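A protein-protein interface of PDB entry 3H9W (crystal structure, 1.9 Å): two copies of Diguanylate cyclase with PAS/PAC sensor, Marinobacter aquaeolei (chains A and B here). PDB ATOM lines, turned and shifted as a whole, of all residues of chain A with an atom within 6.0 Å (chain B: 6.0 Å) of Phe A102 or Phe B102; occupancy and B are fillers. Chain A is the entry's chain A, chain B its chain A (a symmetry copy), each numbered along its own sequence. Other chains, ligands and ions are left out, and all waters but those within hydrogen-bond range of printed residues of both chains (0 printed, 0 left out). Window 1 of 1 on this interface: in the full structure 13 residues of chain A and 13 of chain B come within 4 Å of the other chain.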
ATOM      1  N   ALA A   4      25.835   0.092  -2.309  1.00  0.00           N
ATOM      2  CA  ALA A   4      24.611  -0.610  -1.933  1.00  0.00           C
ATOM      3  C   ALA A   4      23.585  -0.427  -3.043  1.00  0.00           C
ATOM      4  O   ALA A   4      23.520   0.624  -3.674  1.00  0.00           O
ATOM      5  CB  ALA A   4      24.069  -0.059  -0.628  1.00  0.00           C
ATOM      6  N   ILE A   5      22.788  -1.458  -3.286  1.00  0.00           N
ATOM      7  CA  ILE A   5      21.780  -1.399  -4.329  1.00  0.00           C
ATOM      8  C   ILE A   5      20.400  -1.412  -3.705  1.00  0.00           C
ATOM      9  O   ILE A   5      19.972  -2.425  -3.151  1.00  0.00           O
ATOM     10  CB  ILE A   5      21.892  -2.604  -5.281  1.00  0.00           C
ATOM     11  CG1 ILE A   5      23.304  -2.667  -5.867  1.00  0.00           C
ATOM     12  CG2 ILE A   5      20.866  -2.474  -6.395  1.00  0.00           C
ATOM     13  CD1 ILE A   5      23.650  -4.004  -6.485  1.00  0.00           C
ATOM     14  N   PRO A   6      19.686  -0.281  -3.778  1.00  0.00           N
ATOM     15  CA  PRO A   6      18.343  -0.193  -3.210  1.00  0.00           C
ATOM     16  C   PRO A   6      17.321  -0.861  -4.120  1.00  0.00           C
ATOM     17  O   PRO A   6      17.488  -0.881  -5.342  1.00  0.00           O
ATOM     18  CB  PRO A   6      18.122   1.313  -3.095  1.00  0.00           C
ATOM     19  CG  PRO A   6      18.838   1.832  -4.314  1.00  0.00           C
ATOM     20  CD  PRO A   6      20.129   1.027  -4.300  1.00  0.00           C
ATOM     21  N   TRP A   7      16.278  -1.424  -3.521  1.00  0.00           N
ATOM     22  CA  TRP A   7      15.220  -2.066  -4.293  1.00  0.00           C
ATOM     23  C   TRP A   7      13.947  -2.169  -3.461  1.00  0.00           C
ATOM     24  O   TRP A   7      13.978  -2.057  -2.231  1.00  0.00           O
ATOM     25  CB  TRP A   7      15.648  -3.464  -4.751  1.00  0.00           C
ATOM     26  CG  TRP A   7      15.986  -4.376  -3.626  1.00  0.00           C
ATOM     27  CD1 TRP A   7      17.224  -4.603  -3.092  1.00  0.00           C
ATOM     28  CD2 TRP A   7      15.062  -5.138  -2.839  1.00  0.00           C
ATOM     29  NE1 TRP A   7      17.126  -5.460  -2.016  1.00  0.00           N
ATOM     30  CE2 TRP A   7      15.809  -5.802  -1.840  1.00  0.00           C
ATOM     31  CE3 TRP A   7      13.672  -5.324  -2.882  1.00  0.00           C
ATOM     32  CZ2 TRP A   7      15.216  -6.628  -0.890  1.00  0.00           C
ATOM     33  CZ3 TRP A   7      13.080  -6.149  -1.937  1.00  0.00           C
ATOM     34  CH2 TRP A   7      13.856  -6.794  -0.952  1.00  0.00           C
ATOM     35  N   ASP A  65      11.490  -9.437   9.123  1.00  0.00           N
ATOM     36  CA  ASP A  65      12.643  -8.949   8.368  1.00  0.00           C
ATOM     37  C   ASP A  65      13.669 -10.052   8.318  1.00  0.00           C
ATOM     38  O   ASP A  65      13.795 -10.828   9.258  1.00  0.00           O
ATOM     39  CB  ASP A  65      13.258  -7.727   9.038  1.00  0.00           C
ATOM     40  CG  ASP A  65      12.411  -6.499   8.870  1.00  0.00           C
ATOM     41  OD1 ASP A  65      11.242  -6.639   8.448  1.00  0.00           O
ATOM     42  OD2 ASP A  65      12.916  -5.401   9.161  1.00  0.00           O
ATOM     43  N   ARG A  83      24.629 -10.058  -0.412  1.00  0.00           N
ATOM     44  CA  ARG A  83      23.866 -10.133   0.820  1.00  0.00           C
ATOM     45  C   ARG A  83      22.620  -9.313   0.519  1.00  0.00           C
ATOM     46  O   ARG A  83      22.716  -8.141   0.162  1.00  0.00           O
ATOM     47  CB  ARG A  83      24.619  -9.503   2.000  1.00  0.00           C
ATOM     48  CG  ARG A  83      23.776  -9.385   3.290  1.00  0.00           C
ATOM     49  CD  ARG A  83      24.665  -9.159   4.516  1.00  0.00           C
ATOM     50  NE  ARG A  83      25.580 -10.289   4.661  1.00  0.00           N
ATOM     51  CZ  ARG A  83      26.885 -10.193   4.892  1.00  0.00           C
ATOM     52  NH1 ARG A  83      27.464  -9.005   5.025  1.00  0.00           N
ATOM     53  NH2 ARG A  83      27.618 -11.297   4.939  1.00  0.00           N
ATOM     54  N   ASP A  84      21.459  -9.942   0.640  1.00  0.00           N
ATOM     55  CA  ASP A  84      20.197  -9.267   0.390  1.00  0.00           C
ATOM     56  C   ASP A  84      19.580  -9.052   1.776  1.00  0.00           C
ATOM     57  O   ASP A  84      19.430 -10.004   2.547  1.00  0.00           O
ATOM     58  CB  ASP A  84      19.316 -10.164  -0.490  1.00  0.00           C
ATOM     59  CG  ASP A  84      18.103  -9.447  -1.051  1.00  0.00           C
ATOM     60  OD1 ASP A  84      17.995  -8.215  -0.903  1.00  0.00           O
ATOM     61  OD2 ASP A  84      17.250 -10.131  -1.661  1.00  0.00           O
ATOM     62  N   VAL A  85      19.263  -7.798   2.095  1.00  0.00           N
ATOM     63  CA  VAL A  85      18.681  -7.430   3.384  1.00  0.00           C
ATOM     64  C   VAL A  85      17.286  -6.911   3.124  1.00  0.00           C
ATOM     65  O   VAL A  85      17.102  -5.975   2.348  1.00  0.00           O
ATOM     66  CB  VAL A  85      19.506  -6.337   4.083  1.00  0.00           C
ATOM     67  CG1 VAL A  85      18.896  -6.016   5.444  1.00  0.00           C
ATOM     68  CG2 VAL A  85      20.943  -6.812   4.251  1.00  0.00           C
ATOM     69  N   VAL A  86      16.314  -7.516   3.799  1.00  0.00           N
ATOM     70  CA  VAL A  86      14.914  -7.198   3.576  1.00  0.00           C
ATOM     71  C   VAL A  86      14.091  -6.735   4.761  1.00  0.00           C
ATOM     72  O   VAL A  86      14.083  -7.367   5.818  1.00  0.00           O
ATOM     73  CB  VAL A  86      14.177  -8.426   2.995  1.00  0.00           C
ATOM     74  CG1 VAL A  86      12.768  -8.037   2.581  1.00  0.00           C
ATOM     75  CG2 VAL A  86      14.960  -8.984   1.809  1.00  0.00           C
ATOM     76  N   HIS A  87      13.383  -5.630   4.558  1.00  0.00           N
ATOM     77  CA  HIS A  87      12.482  -5.102   5.567  1.00  0.00           C
ATOM     78  C   HIS A  87      11.083  -5.324   4.997  1.00  0.00           C
ATOM     79  O   HIS A  87      10.834  -5.003   3.835  1.00  0.00           O
ATOM     80  CB  HIS A  87      12.703  -3.611   5.789  1.00  0.00           C
ATOM     81  CG  HIS A  87      11.663  -2.988   6.667  1.00  0.00           C
ATOM     82  ND1 HIS A  87      10.822  -1.989   6.230  1.00  0.00           N
ATOM     83  CD2 HIS A  87      11.289  -3.265   7.939  1.00  0.00           C
ATOM     84  CE1 HIS A  87       9.972  -1.678   7.193  1.00  0.00           C
ATOM     85  NE2 HIS A  87      10.234  -2.438   8.240  1.00  0.00           N
ATOM     86  N   ILE A 100      11.189  -3.948   1.040  1.00  0.00           N
ATOM     87  CA  ILE A 100      12.137  -2.890   0.703  1.00  0.00           C
ATOM     88  C   ILE A 100      13.488  -3.229   1.315  1.00  0.00           C
ATOM     89  O   ILE A 100      13.559  -3.688   2.452  1.00  0.00           O
ATOM     90  CB  ILE A 100      11.694  -1.530   1.284  1.00  0.00           C
ATOM     91  CG1 ILE A 100      11.676  -1.614   2.814  1.00  0.00           C
ATOM     92  CG2 ILE A 100      10.306  -1.178   0.788  1.00  0.00           C
ATOM     93  CD1 ILE A 100      11.722  -0.271   3.515  1.00  0.00           C
ATOM     94  N   GLY A 101      14.562  -2.992   0.580  1.00  0.00           N
ATOM     95  CA  GLY A 101      15.857  -3.300   1.143  1.00  0.00           C
ATOM     96  C   GLY A 101      17.022  -2.920   0.271  1.00  0.00           C
ATOM     97  O   GLY A 101      16.918  -2.045  -0.591  1.00  0.00           O
ATOM     98  N   PHE A 102      18.141  -3.595   0.499  1.00  0.00           N
ATOM     99  CA  PHE A 102      19.358  -3.338  -0.255  1.00  0.00           C
ATOM    100  C   PHE A 102      20.067  -4.644  -0.576  1.00  0.00           C
ATOM    101  O   PHE A 102      19.961  -5.615   0.167  1.00  0.00           O
ATOM    102  CB  PHE A 102      20.342  -2.503   0.575  1.00  0.00           C
ATOM    103  CG  PHE A 102      19.913  -1.086   0.825  1.00  0.00           C
ATOM    104  CD1 PHE A 102      20.109  -0.109  -0.135  1.00  0.00           C
ATOM    105  CD2 PHE A 102      19.355  -0.723   2.046  1.00  0.00           C
ATOM    106  CE1 PHE A 102      19.757   1.225   0.118  1.00  0.00           C
ATOM    107  CE2 PHE A 102      18.998   0.605   2.309  1.00  0.00           C
ATOM    108  CZ  PHE A 102      19.203   1.573   1.339  1.00  0.00           C
ATOM    109  N   MET A 103      20.796  -4.646  -1.686  1.00  0.00           N
ATOM    110  CA  MET A 103      21.616  -5.784  -2.070  1.00  0.00           C
ATOM    111  C   MET A 103      23.029  -5.241  -1.944  1.00  0.00           C
ATOM    112  O   MET A 103      23.312  -4.123  -2.375  1.00  0.00           O
ATOM    113  CB  MET A 103      21.344  -6.217  -3.510  1.00  0.00           C
ATOM    114  CG  MET A 103      20.209  -7.201  -3.642  1.00  0.00           C
ATOM    115  SD  MET A 103      19.641  -7.353  -5.477  1.00  0.00           S
ATOM    116  CE  MET A 103      17.782  -7.703  -5.128  1.00  0.00           C
ATOM    117  N   PHE A 104      23.907  -6.034  -1.341  1.00  0.00           N
ATOM    118  CA  PHE A 104      25.291  -5.631  -1.120  1.00  0.00           C
ATOM    119  C   PHE A 104      26.263  -6.634  -1.719  1.00  0.00           C
ATOM    120  O   PHE A 104      26.068  -7.844  -1.595  1.00  0.00           O
ATOM    121  CB  PHE A 104      25.575  -5.565   0.380  1.00  0.00           C
ATOM    122  CG  PHE A 104      24.729  -4.576   1.125  1.00  0.00           C
ATOM    123  CD1 PHE A 104      25.078  -3.230   1.154  1.00  0.00           C
ATOM    124  CD2 PHE A 104      23.591  -4.991   1.814  1.00  0.00           C
ATOM    125  CE1 PHE A 104      24.306  -2.311   1.863  1.00  0.00           C
ATOM    126  CE2 PHE A 104      22.812  -4.079   2.527  1.00  0.00           C
ATOM    127  CZ  PHE A 104      23.172  -2.737   2.550  1.00  0.00           C
ATOM    128  N   ALA B   4      20.703  -6.827  11.006  1.00  0.00           N
ATOM    129  CA  ALA B   4      20.506  -5.513  10.400  1.00  0.00           C
ATOM    130  C   ALA B   4      19.412  -4.785  11.167  1.00  0.00           C
ATOM    131  O   ALA B   4      18.453  -5.396  11.632  1.00  0.00           O
ATOM    132  CB  ALA B   4      20.110  -5.662   8.944  1.00  0.00           C
ATOM    133  N   ILE B   5      19.559  -3.475  11.305  1.00  0.00           N
ATOM    134  CA  ILE B   5      18.582  -2.680  12.026  1.00  0.00           C
ATOM    135  C   ILE B   5      17.860  -1.762  11.063  1.00  0.00           C
ATOM    136  O   ILE B   5      18.449  -0.818  10.534  1.00  0.00           O
ATOM    137  CB  ILE B   5      19.257  -1.813  13.106  1.00  0.00           C
ATOM    138  CG1 ILE B   5      20.064  -2.705  14.051  1.00  0.00           C
ATOM    139  CG2 ILE B   5      18.198  -1.046  13.883  1.00  0.00           C
ATOM    140  CD1 ILE B   5      21.074  -1.951  14.888  1.00  0.00           C
ATOM    141  N   PRO B   6      16.572  -2.032  10.812  1.00  0.00           N
ATOM    142  CA  PRO B   6      15.786  -1.205   9.899  1.00  0.00           C
ATOM    143  C   PRO B   6      15.352   0.089  10.573  1.00  0.00           C
ATOM    144  O   PRO B   6      15.148   0.125  11.789  1.00  0.00           O
ATOM    145  CB  PRO B   6      14.603  -2.107   9.556  1.00  0.00           C
ATOM    146  CG  PRO B   6      14.376  -2.836  10.855  1.00  0.00           C
ATOM    147  CD  PRO B   6      15.792  -3.195  11.279  1.00  0.00           C
ATOM    148  N   TRP B   7      15.233   1.152   9.786  1.00  0.00           N
ATOM    149  CA  TRP B   7      14.793   2.438  10.316  1.00  0.00           C
ATOM    150  C   TRP B   7      14.260   3.319   9.191  1.00  0.00           C
ATOM    151  O   TRP B   7      14.529   3.077   8.010  1.00  0.00           O
ATOM    152  CB  TRP B   7      15.943   3.158  11.029  1.00  0.00           C
ATOM    153  CG  TRP B   7      17.112   3.422  10.148  1.00  0.00           C
ATOM    154  CD1 TRP B   7      18.221   2.639   9.994  1.00  0.00           C
ATOM    155  CD2 TRP B   7      17.261   4.517   9.235  1.00  0.00           C
ATOM    156  NE1 TRP B   7      19.054   3.180   9.036  1.00  0.00           N
ATOM    157  CE2 TRP B   7      18.485   4.333   8.556  1.00  0.00           C
ATOM    158  CE3 TRP B   7      16.476   5.639   8.927  1.00  0.00           C
ATOM    159  CZ2 TRP B   7      18.940   5.219   7.584  1.00  0.00           C
ATOM    160  CZ3 TRP B   7      16.929   6.523   7.960  1.00  0.00           C
ATOM    161  CH2 TRP B   7      18.155   6.306   7.298  1.00  0.00           C
ATOM    162  N   ASP B  65      21.184   8.665  -2.669  1.00  0.00           N
ATOM    163  CA  ASP B  65      21.387   7.594  -1.695  1.00  0.00           C
ATOM    164  C   ASP B  65      22.825   7.637  -1.247  1.00  0.00           C
ATOM    165  O   ASP B  65      23.710   7.978  -2.023  1.00  0.00           O
ATOM    166  CB  ASP B  65      21.098   6.231  -2.313  1.00  0.00           C
ATOM    167  CG  ASP B  65      19.630   5.999  -2.519  1.00  0.00           C
ATOM    168  OD1 ASP B  65      18.856   6.976  -2.411  1.00  0.00           O
ATOM    169  OD2 ASP B  65      19.256   4.845  -2.788  1.00  0.00           O
ATOM    170  N   ARG B  83      27.634   0.860  10.036  1.00  0.00           N
ATOM    171  CA  ARG B  83      27.520   1.312   8.662  1.00  0.00           C
ATOM    172  C   ARG B  83      26.046   1.662   8.522  1.00  0.00           C
ATOM    173  O   ARG B  83      25.180   0.821   8.755  1.00  0.00           O
ATOM    174  CB  ARG B  83      27.879   0.204   7.662  1.00  0.00           C
ATOM    175  CG  ARG B  83      27.590   0.573   6.188  1.00  0.00           C
ATOM    176  CD  ARG B  83      28.337  -0.356   5.227  1.00  0.00           C
ATOM    177  NE  ARG B  83      29.774  -0.238   5.463  1.00  0.00           N
ATOM    178  CZ  ARG B  83      30.616  -1.258   5.580  1.00  0.00           C
ATOM    179  NH1 ARG B  83      30.185  -2.510   5.470  1.00  0.00           N
ATOM    180  NH2 ARG B  83      31.891  -1.018   5.857  1.00  0.00           N
ATOM    181  N   ASP B  84      25.769   2.909   8.169  1.00  0.00           N
ATOM    182  CA  ASP B  84      24.400   3.366   7.993  1.00  0.00           C
ATOM    183  C   ASP B  84      24.217   3.496   6.478  1.00  0.00           C
ATOM    184  O   ASP B  84      25.001   4.175   5.810  1.00  0.00           O
ATOM    185  CB  ASP B  84      24.229   4.717   8.703  1.00  0.00           C
ATOM    186  CG  ASP B  84      22.780   5.145   8.833  1.00  0.00           C
ATOM    187  OD1 ASP B  84      21.874   4.347   8.521  1.00  0.00           O
ATOM    188  OD2 ASP B  84      22.547   6.295   9.267  1.00  0.00           O
ATOM    189  N   VAL B  85      23.205   2.813   5.943  1.00  0.00           N
ATOM    190  CA  VAL B  85      22.908   2.823   4.512  1.00  0.00           C
ATOM    191  C   VAL B  85      21.562   3.483   4.328  1.00  0.00           C
ATOM    192  O   VAL B  85      20.570   3.054   4.914  1.00  0.00           O
ATOM    193  CB  VAL B  85      22.856   1.398   3.939  1.00  0.00           C
ATOM    194  CG1 VAL B  85      22.595   1.452   2.436  1.00  0.00           C
ATOM    195  CG2 VAL B  85      24.175   0.687   4.216  1.00  0.00           C
ATOM    196  N   VAL B  86      21.539   4.517   3.493  1.00  0.00           N
ATOM    197  CA  VAL B  86      20.341   5.316   3.296  1.00  0.00           C
ATOM    198  C   VAL B  86      19.794   5.442   1.889  1.00  0.00           C
ATOM    199  O   VAL B  86      20.519   5.766   0.947  1.00  0.00           O
ATOM    200  CB  VAL B  86      20.579   6.759   3.796  1.00  0.00           C
ATOM    201  CG1 VAL B  86      19.274   7.536   3.770  1.00  0.00           C
ATOM    202  CG2 VAL B  86      21.169   6.726   5.204  1.00  0.00           C
ATOM    203  N   HIS B  87      18.494   5.201   1.766  1.00  0.00           N
ATOM    204  CA  HIS B  87      17.801   5.358   0.500  1.00  0.00           C
ATOM    205  C   HIS B  87      16.895   6.572   0.696  1.00  0.00           C
ATOM    206  O   HIS B  87      16.196   6.660   1.705  1.00  0.00           O
ATOM    207  CB  HIS B  87      16.946   4.140   0.175  1.00  0.00           C
ATOM    208  CG  HIS B  87      16.060   4.345  -1.015  1.00  0.00           C
ATOM    209  ND1 HIS B  87      14.686   4.299  -0.936  1.00  0.00           N
ATOM    210  CD2 HIS B  87      16.354   4.657  -2.299  1.00  0.00           C
ATOM    211  CE1 HIS B  87      14.170   4.577  -2.121  1.00  0.00           C
ATOM    212  NE2 HIS B  87      15.159   4.797  -2.965  1.00  0.00           N
ATOM    213  N   ILE B 100      14.930   5.995   4.353  1.00  0.00           N
ATOM    214  CA  ILE B 100      14.706   4.626   4.807  1.00  0.00           C
ATOM    215  C   ILE B 100      15.990   3.831   4.621  1.00  0.00           C
ATOM    216  O   ILE B 100      16.666   3.970   3.605  1.00  0.00           O
ATOM    217  CB  ILE B 100      13.607   3.930   3.977  1.00  0.00           C
ATOM    218  CG1 ILE B 100      14.064   3.825   2.518  1.00  0.00           C
ATOM    219  CG2 ILE B 100      12.320   4.728   4.040  1.00  0.00           C
ATOM    220  CD1 ILE B 100      13.326   2.779   1.705  1.00  0.00           C
ATOM    221  N   GLY B 101      16.325   2.989   5.584  1.00  0.00           N
ATOM    222  CA  GLY B 101      17.537   2.218   5.427  1.00  0.00           C
ATOM    223  C   GLY B 101      17.793   1.226   6.528  1.00  0.00           C
ATOM    224  O   GLY B 101      16.873   0.792   7.225  1.00  0.00           O
ATOM    225  N   PHE B 102      19.062   0.876   6.688  1.00  0.00           N
ATOM    226  CA  PHE B 102      19.471  -0.081   7.704  1.00  0.00           C
ATOM    227  C   PHE B 102      20.775   0.359   8.351  1.00  0.00           C
ATOM    228  O   PHE B 102      21.594   1.023   7.724  1.00  0.00           O
ATOM    229  CB  PHE B 102      19.740  -1.455   7.077  1.00  0.00           C
ATOM    230  CG  PHE B 102      18.522  -2.163   6.561  1.00  0.00           C
ATOM    231  CD1 PHE B 102      17.699  -2.871   7.419  1.00  0.00           C
ATOM    232  CD2 PHE B 102      18.227  -2.160   5.202  1.00  0.00           C
ATOM    233  CE1 PHE B 102      16.589  -3.576   6.930  1.00  0.00           C
ATOM    234  CE2 PHE B 102      17.121  -2.859   4.701  1.00  0.00           C
ATOM    235  CZ  PHE B 102      16.308  -3.566   5.574  1.00  0.00           C
ATOM    236  N   MET B 103      20.954  -0.029   9.608  1.00  0.00           N
ATOM    237  CA  MET B 103      22.194   0.223  10.326  1.00  0.00           C
ATOM    238  C   MET B 103      22.762  -1.173  10.520  1.00  0.00           C
ATOM    239  O   MET B 103      22.037  -2.100  10.880  1.00  0.00           O
ATOM    240  CB  MET B 103      21.939   0.881  11.680  1.00  0.00           C
ATOM    241  CG  MET B 103      21.863   2.386  11.617  1.00  0.00           C
ATOM    242  SD  MET B 103      21.111   3.107  13.238  1.00  0.00           S
ATOM    243  CE  MET B 103      20.243   4.630  12.448  1.00  0.00           C
ATOM    244  N   PHE B 104      24.058  -1.316  10.269  1.00  0.00           N
ATOM    245  CA  PHE B 104      24.732  -2.604  10.381  1.00  0.00           C
ATOM    246  C   PHE B 104      25.917  -2.528  11.329  1.00  0.00           C
ATOM    247  O   PHE B 104      26.683  -1.564  11.297  1.00  0.00           O
ATOM    248  CB  PHE B 104      25.271  -3.023   9.014  1.00  0.00           C
ATOM    249  CG  PHE B 104      24.216  -3.195   7.962  1.00  0.00           C
ATOM    250  CD1 PHE B 104      23.495  -4.381   7.872  1.00  0.00           C
ATOM    251  CD2 PHE B 104      23.954  -2.177   7.046  1.00  0.00           C
ATOM    252  CE1 PHE B 104      22.529  -4.553   6.882  1.00  0.00           C
ATOM    253  CE2 PHE B 104      22.990  -2.339   6.051  1.00  0.00           C
ATOM    254  CZ  PHE B 104      22.277  -3.530   5.971  1.00  0.00           C
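The backbone carbonyl oxygen (O) of Trp A7 is in hydrogen-bond range of the backbone NH (N) of Gly A101 (3.0 Å).
The backbone carbonyl oxygen of Arg A83 is in hydrogen-bond range of the backbone NH of Phe A104 (2.8 Å).
O of Phe A102 is in hydrogen-bond range of N of Val A85 (3.0 Å).
O of Ile A100 lies within hydrogen-bond range of N of His A87, 2.9 Å away.
The backbone NH of Gly B101 lies within hydrogen-bond range of the backbone carbonyl oxygen of Trp B7.
The backbone carbonyl oxygen of Phe B102 lies within hydrogen-bond range of the backbone NH of Val B85, at 3.0 Å.
Among the printed residues, merely in contact across the chains: Ala A4 with Val B85, Pro A6 with Asp B65, Pro A6 with His B87, Asp A65 with Pro B6, Val A85 with Ala B4, Val A85 with Phe B102, Val A85 with Phe B104, Val A86 with Phe B102, His A87 with Pro B6, His A87 with Phe B102, Ile A100 with Ile B100, Gly A101 with Phe B102, Phe A102 with Val B85, Phe A102 with Val B86, Phe A102 with His B87, Phe A102 with Gly B101, Phe A102 with Phe B102, Phe A104 with Val B85 and Phe A104 with Phe B104.
Printed residues of chain B within 4 Å of Pro A6: Asp B65 (3.4 Å) and His B87 (3.9 Å).
Of chain B, only Val B85, Val B86, His B87, Gly B101 and Phe B102 come within 4 Å of Phe A102.
Arg B83 touches none of the printed residues of chain A.
Of the printed residues of chain A, Ile B100 touches Ile A100 (3.9 Å).
The nearest residue of chain B that does not touch Phe A102 is Ile B100 (4.2 Å).
The nearest residue of chain A that does not touch Phe B102 is Ile A100 (4.2 Å).
The nearest printed residue of chain B that does not touch His A87 is Trp B7 (6.2 Å).
Printed residues of chain B that touch a printed residue of chain A: Ala B4, Pro B6, Asp B65, Val B85, Val B86, His B87, Ile B100, Gly B101, Phe B102 and Phe B104.
Of the 15 printed residues of chain A, 10 touch a printed residue of chain B.
Printed residues of chain A that touch a printed residue of chain B: Ala A4, Pro A6, Asp A65, Val A85, Val A86, His A87, Ile A100, Gly A101, Phe A102 and Phe A104.
Hydrophobic or aromatic side chains of chain A that line the printed part of chain B: Ala A4, Pro A6, Val A85, His A87, Ile A100, Phe A102 and Phe A104.
Along chain A the printed residues that touch a printed residue of chain B span positions 4 to 104.
Among the printed residues, 19 pairs touch across the chains.
Pro A6 touches His B87, and with the chains exchanged His A87 touches Pro B6.
Val A86 touches Phe B102, and with the chains exchanged Phe A102 touches Val B86.
His A87 touches Phe B102, and with the chains exchanged Phe A102 touches His B87.
Phe A104 touches its own counterpart, Phe B104.
Positions printed for both chains: 4, 5, 6, 7, 65, 83, 84, 85, 86, 87, 100, 101, 102, 103 and 104.
Of the 19 pairs that touch across the chains among the printed residues, 19 have their exchanged pair printed and touching as well.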
